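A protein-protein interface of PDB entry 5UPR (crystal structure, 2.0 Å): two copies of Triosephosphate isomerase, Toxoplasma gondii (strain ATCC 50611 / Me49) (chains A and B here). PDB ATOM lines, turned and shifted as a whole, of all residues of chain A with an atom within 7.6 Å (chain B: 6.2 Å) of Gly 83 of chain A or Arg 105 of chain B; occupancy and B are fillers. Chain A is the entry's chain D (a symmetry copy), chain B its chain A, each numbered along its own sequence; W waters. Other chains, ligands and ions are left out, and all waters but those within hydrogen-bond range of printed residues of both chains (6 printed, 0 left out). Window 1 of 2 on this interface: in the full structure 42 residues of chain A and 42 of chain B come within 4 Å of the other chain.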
ATOM      1  N   ASP A  71      24.167  27.368   2.846  1.00  0.00           N
ATOM      2  CA  ASP A  71      24.331  27.432   1.366  1.00  0.00           C
ATOM      3  C   ASP A  71      24.390  28.881   1.046  1.00  0.00           C
ATOM      4  O   ASP A  71      24.065  29.737   1.908  1.00  0.00           O
ATOM      5  CB  ASP A  71      23.096  26.816   0.676  1.00  0.00           C
ATOM      6  CG  ASP A  71      23.222  26.674  -0.854  1.00  0.00           C
ATOM      7  OD1 ASP A  71      24.360  26.553  -1.423  1.00  0.00           O
ATOM      8  OD2 ASP A  71      22.145  26.697  -1.524  1.00  0.00           O
ATOM      9  N   SER A  73      24.058  31.459  -2.838  1.00  0.00           N
ATOM     10  CA  SER A  73      23.687  31.355  -4.233  1.00  0.00           C
ATOM     11  C   SER A  73      24.868  31.477  -5.206  1.00  0.00           C
ATOM     12  O   SER A  73      25.904  32.147  -4.906  1.00  0.00           O
ATOM     13  CB  SER A  73      22.619  32.407  -4.548  1.00  0.00           C
ATOM     14  OG  SER A  73      22.119  32.231  -5.862  1.00  0.00           O
ATOM     15  N   ALA A  80      16.896  39.451  -9.288  1.00  0.00           N
ATOM     16  CA  ALA A  80      15.646  38.719  -9.490  1.00  0.00           C
ATOM     17  C   ALA A  80      15.892  37.188  -9.398  1.00  0.00           C
ATOM     18  O   ALA A  80      15.862  36.458 -10.455  1.00  0.00           O
ATOM     19  CB  ALA A  80      14.988  39.105 -10.811  1.00  0.00           C
ATOM     20  N   PHE A  81      16.192  36.735  -8.167  1.00  0.00           N
ATOM     21  CA  PHE A  81      16.563  35.374  -7.925  1.00  0.00           C
ATOM     22  C   PHE A  81      15.675  34.804  -6.798  1.00  0.00           C
ATOM     23  O   PHE A  81      16.100  34.611  -5.640  1.00  0.00           O
ATOM     24  CB  PHE A  81      18.052  35.246  -7.594  1.00  0.00           C
ATOM     25  CG  PHE A  81      18.934  36.194  -8.370  1.00  0.00           C
ATOM     26  CD1 PHE A  81      18.996  36.129  -9.751  1.00  0.00           C
ATOM     27  CD2 PHE A  81      19.719  37.141  -7.698  1.00  0.00           C
ATOM     28  CE1 PHE A  81      19.776  37.031 -10.469  1.00  0.00           C
ATOM     29  CE2 PHE A  81      20.541  38.004  -8.393  1.00  0.00           C
ATOM     30  CZ  PHE A  81      20.572  37.951  -9.789  1.00  0.00           C
ATOM     31  N   THR A  82      14.445  34.488  -7.178  1.00  0.00           N
ATOM     32  CA  THR A  82      13.434  34.010  -6.216  1.00  0.00           C
ATOM     33  C   THR A  82      13.917  32.785  -5.433  1.00  0.00           C
ATOM     34  O   THR A  82      14.374  31.780  -6.034  1.00  0.00           O
ATOM     35  CB  THR A  82      12.071  33.793  -6.931  1.00  0.00           C
ATOM     36  OG1 THR A  82      11.562  35.088  -7.427  1.00  0.00           O
ATOM     37  CG2 THR A  82      11.078  33.242  -6.028  1.00  0.00           C
ATOM     38  N   GLY A  83      13.874  32.876  -4.113  1.00  0.00           N
ATOM     39  CA  GLY A  83      14.261  31.798  -3.213  1.00  0.00           C
ATOM     40  C   GLY A  83      15.730  31.576  -2.971  1.00  0.00           C
ATOM     41  O   GLY A  83      16.101  30.594  -2.328  1.00  0.00           O
ATOM     42  N   GLU A  84      16.555  32.475  -3.493  1.00  0.00           N
ATOM     43  CA  GLU A  84      18.018  32.433  -3.331  1.00  0.00           C
ATOM     44  C   GLU A  84      18.492  33.481  -2.350  1.00  0.00           C
ATOM     45  O   GLU A  84      17.966  34.590  -2.371  1.00  0.00           O
ATOM     46  CB  GLU A  84      18.703  32.727  -4.729  1.00  0.00           C
ATOM     47  CG  GLU A  84      18.463  31.697  -5.798  1.00  0.00           C
ATOM     48  CD  GLU A  84      19.071  30.355  -5.442  1.00  0.00           C
ATOM     49  OE1 GLU A  84      20.330  30.256  -5.450  1.00  0.00           O
ATOM     50  OE2 GLU A  84      18.298  29.421  -5.182  1.00  0.00           O
ATOM     51  N   LEU A  85      19.471  33.111  -1.521  1.00  0.00           N
ATOM     52  CA  LEU A  85      20.228  34.044  -0.664  1.00  0.00           C
ATOM     53  C   LEU A  85      21.617  34.257  -1.250  1.00  0.00           C
ATOM     54  O   LEU A  85      22.448  33.332  -1.253  1.00  0.00           O
ATOM     55  CB  LEU A  85      20.351  33.493   0.782  1.00  0.00           C
ATOM     56  CG  LEU A  85      19.003  33.048   1.380  1.00  0.00           C
ATOM     57  CD1 LEU A  85      19.178  32.393   2.730  1.00  0.00           C
ATOM     58  CD2 LEU A  85      18.012  34.215   1.504  1.00  0.00           C
ATOM     59  N   SER A  86      21.858  35.450  -1.764  1.00  0.00           N
ATOM     60  CA  SER A  86      23.124  35.786  -2.355  1.00  0.00           C
ATOM     61  C   SER A  86      24.228  36.023  -1.283  1.00  0.00           C
ATOM     62  O   SER A  86      23.937  36.391  -0.130  1.00  0.00           O
ATOM     63  CB  SER A  86      23.012  37.020  -3.250  1.00  0.00           C
ATOM     64  OG  SER A  86      22.636  38.137  -2.511  1.00  0.00           O
ATOM     65  N   ARG A 105      23.554  18.556  -0.873  1.00  0.00           N
ATOM     66  CA  ARG A 105      23.232  19.525  -1.907  1.00  0.00           C
ATOM     67  C   ARG A 105      23.883  19.100  -3.273  1.00  0.00           C
ATOM     68  O   ARG A 105      23.312  19.379  -4.316  1.00  0.00           O
ATOM     69  CB  ARG A 105      23.679  20.929  -1.559  1.00  0.00           C
ATOM     70  CG  ARG A 105      23.056  21.450  -0.234  1.00  0.00           C
ATOM     71  CD  ARG A 105      23.043  22.986  -0.223  1.00  0.00           C
ATOM     72  NE  ARG A 105      22.245  23.534  -1.322  1.00  0.00           N
ATOM     73  CZ  ARG A 105      20.888  23.515  -1.386  1.00  0.00           C
ATOM     74  NH1 ARG A 105      20.141  23.112  -0.387  1.00  0.00           N
ATOM     75  NH2 ARG A 105      20.272  24.021  -2.426  1.00  0.00           N
ATOM     76  N   GLN A 112      15.180  16.850  -8.268  1.00  0.00           N
ATOM     77  CA  GLN A 112      15.862  17.991  -8.919  1.00  0.00           C
ATOM     78  C   GLN A 112      17.368  17.639  -8.908  1.00  0.00           C
ATOM     79  O   GLN A 112      17.887  17.257  -7.879  1.00  0.00           O
ATOM     80  CB  GLN A 112      15.676  19.300  -8.162  1.00  0.00           C
ATOM     81  CG  GLN A 112      16.289  20.470  -8.865  1.00  0.00           C
ATOM     82  CD  GLN A 112      16.134  21.811  -8.081  1.00  0.00           C
ATOM     83  OE1 GLN A 112      15.472  21.874  -7.005  1.00  0.00           O
ATOM     84  NE2 GLN A 112      16.762  22.881  -8.632  1.00  0.00           N
ATOM     85  N   ASN B  15       6.559  39.735  -4.094  1.00  0.00           N
ATOM     86  CA  ASN B  15       7.696  38.862  -4.109  1.00  0.00           C
ATOM     87  C   ASN B  15       8.944  39.794  -4.145  1.00  0.00           C
ATOM     88  O   ASN B  15       9.291  40.316  -5.206  1.00  0.00           O
ATOM     89  CB  ASN B  15       7.670  37.968  -5.351  1.00  0.00           C
ATOM     90  CG  ASN B  15       8.901  37.050  -5.452  1.00  0.00           C
ATOM     91  OD1 ASN B  15       9.721  36.992  -4.518  1.00  0.00           O
ATOM     92  ND2 ASN B  15       9.032  36.319  -6.589  1.00  0.00           N
ATOM     93  N   LYS B  17      11.959  38.890  -3.999  1.00  0.00           N
ATOM     94  CA  LYS B  17      13.067  38.199  -4.617  1.00  0.00           C
ATOM     95  C   LYS B  17      14.362  38.350  -3.791  1.00  0.00           C
ATOM     96  O   LYS B  17      14.269  38.412  -2.537  1.00  0.00           O
ATOM     97  CB  LYS B  17      13.200  38.563  -6.092  1.00  0.00           C
ATOM     98  CG  LYS B  17      11.909  38.449  -6.882  1.00  0.00           C
ATOM     99  CD  LYS B  17      12.089  38.689  -8.391  1.00  0.00           C
ATOM    100  CE  LYS B  17      10.689  38.490  -9.093  1.00  0.00           C
ATOM    101  NZ  LYS B  17      10.856  38.606 -10.589  1.00  0.00           N
ATOM    102  N   CYS B  18      15.525  38.393  -4.438  1.00  0.00           N
ATOM    103  CA  CYS B  18      16.822  38.399  -3.726  1.00  0.00           C
ATOM    104  C   CYS B  18      17.240  39.854  -3.524  1.00  0.00           C
ATOM    105  O   CYS B  18      18.232  40.345  -4.104  1.00  0.00           O
ATOM    106  CB  CYS B  18      17.869  37.552  -4.495  1.00  0.00           C
ATOM    107  SG  CYS B  18      19.409  37.351  -3.573  1.00  0.00           S
ATOM    108  N   GLN B  70       9.755  32.350  -0.084  1.00  0.00           N
ATOM    109  CA  GLN B  70       9.885  32.344  -1.560  1.00  0.00           C
ATOM    110  C   GLN B  70      10.070  30.956  -2.195  1.00  0.00           C
ATOM    111  O   GLN B  70      10.160  30.880  -3.450  1.00  0.00           O
ATOM    112  CB  GLN B  70      11.067  33.253  -1.962  1.00  0.00           C
ATOM    113  CG  GLN B  70      10.842  34.740  -1.694  1.00  0.00           C
ATOM    114  CD  GLN B  70      12.060  35.616  -2.047  1.00  0.00           C
ATOM    115  OE1 GLN B  70      12.962  35.179  -2.834  1.00  0.00           O
ATOM    116  NE2 GLN B  70      12.088  36.855  -1.507  1.00  0.00           N
ATOM    117  N   ASP B  71      10.158  29.896  -1.360  1.00  0.00           N
ATOM    118  CA  ASP B  71      10.359  28.516  -1.833  1.00  0.00           C
ATOM    119  C   ASP B  71      10.127  27.659  -0.616  1.00  0.00           C
ATOM    120  O   ASP B  71      10.076  28.163   0.520  1.00  0.00           O
ATOM    121  CB  ASP B  71      11.787  28.317  -2.333  1.00  0.00           C
ATOM    122  CG  ASP B  71      12.056  26.946  -2.993  1.00  0.00           C
ATOM    123  OD1 ASP B  71      11.154  26.271  -3.527  1.00  0.00           O
ATOM    124  OD2 ASP B  71      13.246  26.526  -2.917  1.00  0.00           O
ATOM    125  N   VAL B  99       5.604  30.643  -1.815  1.00  0.00           N
ATOM    126  CA  VAL B  99       5.625  30.765  -3.267  1.00  0.00           C
ATOM    127  C   VAL B  99       6.322  29.560  -3.843  1.00  0.00           C
ATOM    128  O   VAL B  99       7.453  29.227  -3.410  1.00  0.00           O
ATOM    129  CB  VAL B  99       6.378  32.036  -3.693  1.00  0.00           C
ATOM    130  CG1 VAL B  99       6.405  32.176  -5.218  1.00  0.00           C
ATOM    131  CG2 VAL B  99       5.767  33.319  -2.998  1.00  0.00           C
ATOM    132  N   GLY B 101       7.212  27.188  -7.559  1.00  0.00           N
ATOM    133  CA  GLY B 101       7.307  27.191  -8.995  1.00  0.00           C
ATOM    134  C   GLY B 101       7.487  28.481  -9.765  1.00  0.00           C
ATOM    135  O   GLY B 101       7.181  28.539 -10.947  1.00  0.00           O
ATOM    136  N   HIS B 102       8.045  29.503  -9.110  1.00  0.00           N
ATOM    137  CA  HIS B 102       8.403  30.708  -9.801  1.00  0.00           C
ATOM    138  C   HIS B 102       9.255  30.386 -11.022  1.00  0.00           C
ATOM    139  O   HIS B 102      10.158  29.519 -10.923  1.00  0.00           O
ATOM    140  CB  HIS B 102       9.125  31.695  -8.885  1.00  0.00           C
ATOM    141  CG  HIS B 102       9.111  33.097  -9.410  1.00  0.00           C
ATOM    142  ND1 HIS B 102      10.006  33.542 -10.328  1.00  0.00           N
ATOM    143  CD2 HIS B 102       8.234  34.108  -9.208  1.00  0.00           C
ATOM    144  CE1 HIS B 102       9.709  34.792 -10.635  1.00  0.00           C
ATOM    145  NE2 HIS B 102       8.638  35.164  -9.968  1.00  0.00           N
ATOM    146  N   SER B 103       9.053  31.101 -12.102  1.00  0.00           N
ATOM    147  CA  SER B 103       9.837  30.808 -13.331  1.00  0.00           C
ATOM    148  C   SER B 103      11.347  30.924 -13.133  1.00  0.00           C
ATOM    149  O   SER B 103      12.124  30.203 -13.787  1.00  0.00           O
ATOM    150  CB  SER B 103       9.440  31.666 -14.559  1.00  0.00           C
ATOM    151  OG  SER B 103       9.512  32.976 -14.149  1.00  0.00           O
ATOM    152  N   GLU B 104      11.767  31.794 -12.236  1.00  0.00           N
ATOM    153  CA  GLU B 104      13.221  31.891 -11.948  1.00  0.00           C
ATOM    154  C   GLU B 104      13.756  30.556 -11.356  1.00  0.00           C
ATOM    155  O   GLU B 104      14.846  30.127 -11.751  1.00  0.00           O
ATOM    156  CB  GLU B 104      13.550  33.123 -11.088  1.00  0.00           C
ATOM    157  CG  GLU B 104      13.237  34.432 -11.793  1.00  0.00           C
ATOM    158  CD  GLU B 104      12.900  35.594 -10.886  1.00  0.00           C
ATOM    159  OE1 GLU B 104      13.066  35.469  -9.641  1.00  0.00           O
ATOM    160  OE2 GLU B 104      12.515  36.692 -11.469  1.00  0.00           O
ATOM    161  N   ARG B 105      12.969  29.879 -10.528  1.00  0.00           N
ATOM    162  CA  ARG B 105      13.371  28.599  -9.920  1.00  0.00           C
ATOM    163  C   ARG B 105      13.134  27.446 -10.899  1.00  0.00           C
ATOM    164  O   ARG B 105      13.879  26.478 -10.840  1.00  0.00           O
ATOM    165  CB  ARG B 105      12.639  28.329  -8.602  1.00  0.00           C
ATOM    166  CG  ARG B 105      12.860  29.424  -7.532  1.00  0.00           C
ATOM    167  CD  ARG B 105      12.643  28.895  -6.142  1.00  0.00           C
ATOM    168  NE  ARG B 105      13.599  27.806  -5.811  1.00  0.00           N
ATOM    169  CZ  ARG B 105      14.902  27.962  -5.515  1.00  0.00           C
ATOM    170  NH1 ARG B 105      15.447  29.179  -5.381  1.00  0.00           N
ATOM    171  NH2 ARG B 105      15.631  26.904  -5.226  1.00  0.00           N
ATOM    172  N   ARG B 106      12.120  27.534 -11.787  1.00  0.00           N
ATOM    173  CA  ARG B 106      11.950  26.530 -12.835  1.00  0.00           C
ATOM    174  C   ARG B 106      13.143  26.574 -13.804  1.00  0.00           C
ATOM    175  O   ARG B 106      13.598  25.506 -14.257  1.00  0.00           O
ATOM    176  CB  ARG B 106      10.635  26.656 -13.631  1.00  0.00           C
ATOM    177  CG  ARG B 106       9.385  26.369 -12.794  1.00  0.00           C
ATOM    178  CD  ARG B 106       8.082  26.772 -13.540  1.00  0.00           C
ATOM    179  NE  ARG B 106       6.860  26.513 -12.830  1.00  0.00           N
ATOM    180  CZ  ARG B 106       6.099  25.384 -12.881  1.00  0.00           C
ATOM    181  NH1 ARG B 106       6.470  24.318 -13.537  1.00  0.00           N
ATOM    182  NH2 ARG B 106       4.958  25.341 -12.229  1.00  0.00           N
ATOM    183  N   ALA B 107      13.699  27.749 -14.067  1.00  0.00           N
ATOM    184  CA  ALA B 107      14.822  27.850 -15.002  1.00  0.00           C
ATOM    185  C   ALA B 107      16.145  27.422 -14.362  1.00  0.00           C
ATOM    186  O   ALA B 107      17.032  26.917 -15.034  1.00  0.00           O
ATOM    187  CB  ALA B 107      14.980  29.273 -15.563  1.00  0.00           C
ATOM    188  N   GLY B 108      16.293  27.666 -13.076  1.00  0.00           N
ATOM    189  CA  GLY B 108      17.494  27.303 -12.353  1.00  0.00           C
ATOM    190  C   GLY B 108      18.540  28.421 -12.426  1.00  0.00           C
ATOM    191  O   GLY B 108      18.380  29.377 -13.124  1.00  0.00           O
ATOM    192  N   PHE B 109      19.592  28.261 -11.644  1.00  0.00           N
ATOM    193  CA  PHE B 109      20.611  29.251 -11.389  1.00  0.00           C
ATOM    194  C   PHE B 109      22.022  28.748 -11.583  1.00  0.00           C
ATOM    195  O   PHE B 109      22.456  27.701 -10.988  1.00  0.00           O
ATOM    196  CB  PHE B 109      20.479  29.731  -9.942  1.00  0.00           C
ATOM    197  CG  PHE B 109      19.091  30.238  -9.568  1.00  0.00           C
ATOM    198  CD1 PHE B 109      18.653  31.505  -9.989  1.00  0.00           C
ATOM    199  CD2 PHE B 109      18.210  29.432  -8.862  1.00  0.00           C
ATOM    200  CE1 PHE B 109      17.389  31.962  -9.626  1.00  0.00           C
ATOM    201  CE2 PHE B 109      16.974  29.863  -8.520  1.00  0.00           C
ATOM    202  CZ  PHE B 109      16.538  31.161  -8.906  1.00  0.00           C
ATOM    203  N   PRO B 113      20.500  22.689 -12.951  1.00  0.00           N
ATOM    204  CA  PRO B 113      19.152  22.575 -13.482  1.00  0.00           C
ATOM    205  C   PRO B 113      18.100  23.090 -12.508  1.00  0.00           C
ATOM    206  O   PRO B 113      18.277  23.026 -11.314  1.00  0.00           O
ATOM    207  CB  PRO B 113      18.989  21.061 -13.727  1.00  0.00           C
ATOM    208  CG  PRO B 113      20.375  20.580 -13.976  1.00  0.00           C
ATOM    209  CD  PRO B 113      21.250  21.441 -13.073  1.00  0.00           C
ATOM    210  N   GLY B 114      17.031  23.658 -13.043  1.00  0.00           N
ATOM    211  CA  GLY B 114      15.913  24.140 -12.256  1.00  0.00           C
ATOM    212  C   GLY B 114      14.908  23.034 -11.929  1.00  0.00           C
ATOM    213  O   GLY B 114      15.173  21.853 -12.144  1.00  0.00           O
ATOM    214  N   GLU B 115      13.789  23.487 -11.371  1.00  0.00           N
ATOM    215  CA  GLU B 115      12.702  22.610 -10.898  1.00  0.00           C
ATOM    216  C   GLU B 115      11.774  22.277 -12.052  1.00  0.00           C
ATOM    217  O   GLU B 115      11.150  23.171 -12.624  1.00  0.00           O
ATOM    218  CB  GLU B 115      11.902  23.381  -9.817  1.00  0.00           C
ATOM    219  CG  GLU B 115      12.730  23.786  -8.625  1.00  0.00           C
ATOM    220  CD  GLU B 115      12.073  24.748  -7.648  1.00  0.00           C
ATOM    221  OE1 GLU B 115      10.823  25.027  -7.692  1.00  0.00           O
ATOM    222  OE2 GLU B 115      12.911  25.308  -6.873  1.00  0.00           O
ATOM    223  N   SER B 116      11.639  20.991 -12.361  1.00  0.00           N
ATOM    224  CA  SER B 116      10.680  20.519 -13.346  1.00  0.00           C
ATOM    225  C   SER B 116       9.243  20.659 -12.871  1.00  0.00           C
ATOM    226  O   SER B 116       8.981  20.937 -11.659  1.00  0.00           O
ATOM    227  CB  SER B 116      10.935  19.039 -13.615  1.00  0.00           C
ATOM    228  OG  SER B 116      10.588  18.254 -12.469  1.00  0.00           O
ATOM    229  N   LYS B 123       6.823  19.711  -4.352  1.00  0.00           N
ATOM    230  CA  LYS B 123       6.876  20.765  -3.336  1.00  0.00           C
ATOM    231  C   LYS B 123       5.457  21.184  -2.908  1.00  0.00           C
ATOM    232  O   LYS B 123       5.221  21.406  -1.708  1.00  0.00           O
ATOM    233  CB  LYS B 123       7.652  21.965  -3.815  1.00  0.00           C
ATOM    234  CG  LYS B 123       9.122  21.763  -4.033  1.00  0.00           C
ATOM    235  CD  LYS B 123       9.890  22.979  -4.555  1.00  0.00           C
ATOM    236  CE  LYS B 123      11.344  22.705  -4.465  1.00  0.00           C
ATOM    237  NZ  LYS B 123      12.181  23.892  -4.338  1.00  0.00           N
HETATM  238  O   HOH W   1      15.092  23.779  -5.097  1.00  0.00           O
HETATM  239  O   HOH W   2      15.408  26.072  -8.500  1.00  0.00           O
HETATM  240  O   HOH W   3      18.784  26.860  -4.862  1.00  0.00           O
HETATM  241  O   HOH W   4      15.380  35.107  -1.277  1.00  0.00           O
HETATM  242  O   HOH W   5      17.943  25.494  -7.420  1.00  0.00           O
HETATM  243  O   HOH W   6      15.344  27.971  -1.882  1.00  0.00           O
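Water W3 lies within hydrogen-bond range of OE2 of Glu 84 of chain A and NH2 of Arg 105 of chain B.
Water W1 lies within hydrogen-bond range of the side-chain amide oxygen (OE1) of Gln 112 of chain A (2.7 Å), the side-chain amino group (NZ) of Lys 123 of chain B (3.0 Å), the guanidinium group (NH2) of Arg 105 of chain B (3.2 Å) and the side-chain carboxylate (OE2) of Glu 115 of chain B (3.2 Å).
Water W6 bridges the side-chain carboxylate (OD2) of Asp 71 of chain B and the backbone carbonyl oxygen (O) of Gly 83 of chain A.
Water W2 lies within hydrogen-bond range of O of Arg 105 of chain B, OE2 of Glu 115 of chain B and NE2 of Gln 112 of chain A.
Water W4 lies within hydrogen-bond range of the backbone carbonyl oxygen (O) of Glu 84 of chain A and the side-chain amide oxygen (OE1) of Gln 70 of chain B.
Water W5 bridges NE2 of Gln 112 of chain A (3.1 Å) and NH2 of Arg 105 of chain B (3.5 Å).
N of Lys 17 of chain B is in hydrogen-bond range of OD1 of Asn 15 of chain B (3.0 Å).
OE2 of Glu 104 of chain B is in salt-bridge range of NZ of Lys 17 of chain B (2.7 Å).
NE of Arg 105 of chain B lies within salt-bridge range of OD2 of Asp 71 of chain B, at 3.2 Å.
The guanidinium group (NE) of Arg 105 of chain B lies within salt-bridge range of the side-chain carboxylate (OE2) of Glu 115 of chain B (2.8 Å).
OE2 of Glu 115 of chain B lies within salt-bridge range of NZ of Lys 123 of chain B, 3.0 Å away.
The side-chain carboxylate of Glu 84 of chain A sits at hydrogen-bond distance from the side-chain hydroxyl of Ser 73 of chain A (2.7 Å).
The side-chain amide nitrogen of Asn 15 of chain B lies within hydrogen-bond range of the side-chain hydroxyl of Thr 82 of chain A (2.9 Å).
The side-chain sulfur (SG) of Cys 18 of chain B lies within hydrogen-bond range of the backbone carbonyl oxygen (O) of Glu 84 of chain A, 3.3 Å away.
The side-chain hydroxyl (OG) of Ser 86 of chain A is in hydrogen-bond range of the side-chain sulfur (SG) of Cys 18 of chain B, at 3.5 Å.
The side-chain amide oxygen (OE1) of Gln 70 of chain B sits at hydrogen-bond distance from the backbone NH (N) of Gly 83 of chain A (2.8 Å).
The side-chain hydroxyl (OG1) of Thr 82 of chain A lies within hydrogen-bond range of the side-chain carboxylate (OE1) of Glu 104 of chain B, at 2.7 Å.
The backbone carbonyl oxygen (O) of Thr 82 of chain A is in hydrogen-bond range of the guanidinium group (NH1) of Arg 105 of chain B, 2.9 Å away.
The backbone carbonyl oxygen (O) of Gly 83 of chain A lies close to the guanidinium group (NH1) of Arg 105 of chain B, 3.4 Å away.
The side-chain carboxylate of Glu 84 of chain A lies within salt-bridge range of the guanidinium group of Arg 105 of chain B, at 2.9 Å.
The backbone carbonyl oxygen (O) of Pro 113 of chain B lies within hydrogen-bond range of the side-chain amide nitrogen (NE2) of Gln 112 of chain A (3.1 Å).
The side-chain carboxylate (OE1) of Glu 104 of chain B sits close to the backbone carbonyl oxygen (O) of Ala 80 of chain A, at 3.1 Å.
Gly 83 of chain A touches two residues of chain B.
Of the printed residues of chain A, Gln 70 of chain B touches Thr 82 (3.6 Å) and Gly 83 (2.8 Å).
Of the printed residues of chain B, Phe 81 of chain A touches Cys 18, Glu 104 and Phe 109.
Of the printed residues of chain B, Ser 86 of chain A touches Cys 18 (3.5 Å).
Of the printed residues of chain A, Cys 18 of chain B touches Phe 81, Glu 84 and Ser 86.
Of the printed residues of chain B, Ala 80 of chain A touches Lys 17 and Glu 104.
Gly 101 of chain B touches none of the printed residues of chain A.
Ser 73 of chain A touches none of the printed residues of chain B.
The nearest residue of chain B that does not touch Gly 83 of chain A is Asp 71 of chain B (4.4 Å).
The nearest printed residue of chain A that does not touch Pro 113 of chain B is Glu 84 of chain A (8.9 Å).
Ala 80 of chain A touches Lys 17 of chain B.
Phe 81 of chain A touches Cys 18 of chain B (O to CB, 3.6 Å).
OE1 of Glu 104 of chain B touches N of Phe 81 of chain A, at 3.7 Å.
CE1 of Phe 109 of chain B touches CA of Phe 81 of chain A (3.9 Å).
CA of Thr 82 of chain A touches OE1 of Gln 70 of chain B, 3.6 Å away.
OG1 of Thr 82 of chain A touches ND1 of His 102 of chain B, at 3.6 Å.
Phe 109 of chain B touches Thr 82 of chain A.
Phe 109 of chain B touches Glu 84 of chain A.
Gly 114 of chain B touches Gln 112 of chain A (O to CG, 3.7 Å).
Gln 112 of chain A touches Glu 115 of chain B (OE1 to CG, 3.7 Å).
Hydrophobic or aromatic side chains of chain B within 4 Å of the printed part of chain A: His 102 and Phe 109.
Of the 11 printed residues of chain A, 7 touch a printed residue of chain B.
Hydrophobic or aromatic side chains of chain A within 4 Å of the printed part of chain B: Ala 80 and Phe 81.
Among the printed residues, Asp or Glu carboxylates within 4 Å of a Lys or Arg side-chain nitrogen of the other chain: Glu 84 of chain A with Arg 105 of chain B (2.9 Å).
Positions printed for both chains: 71 and 105.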
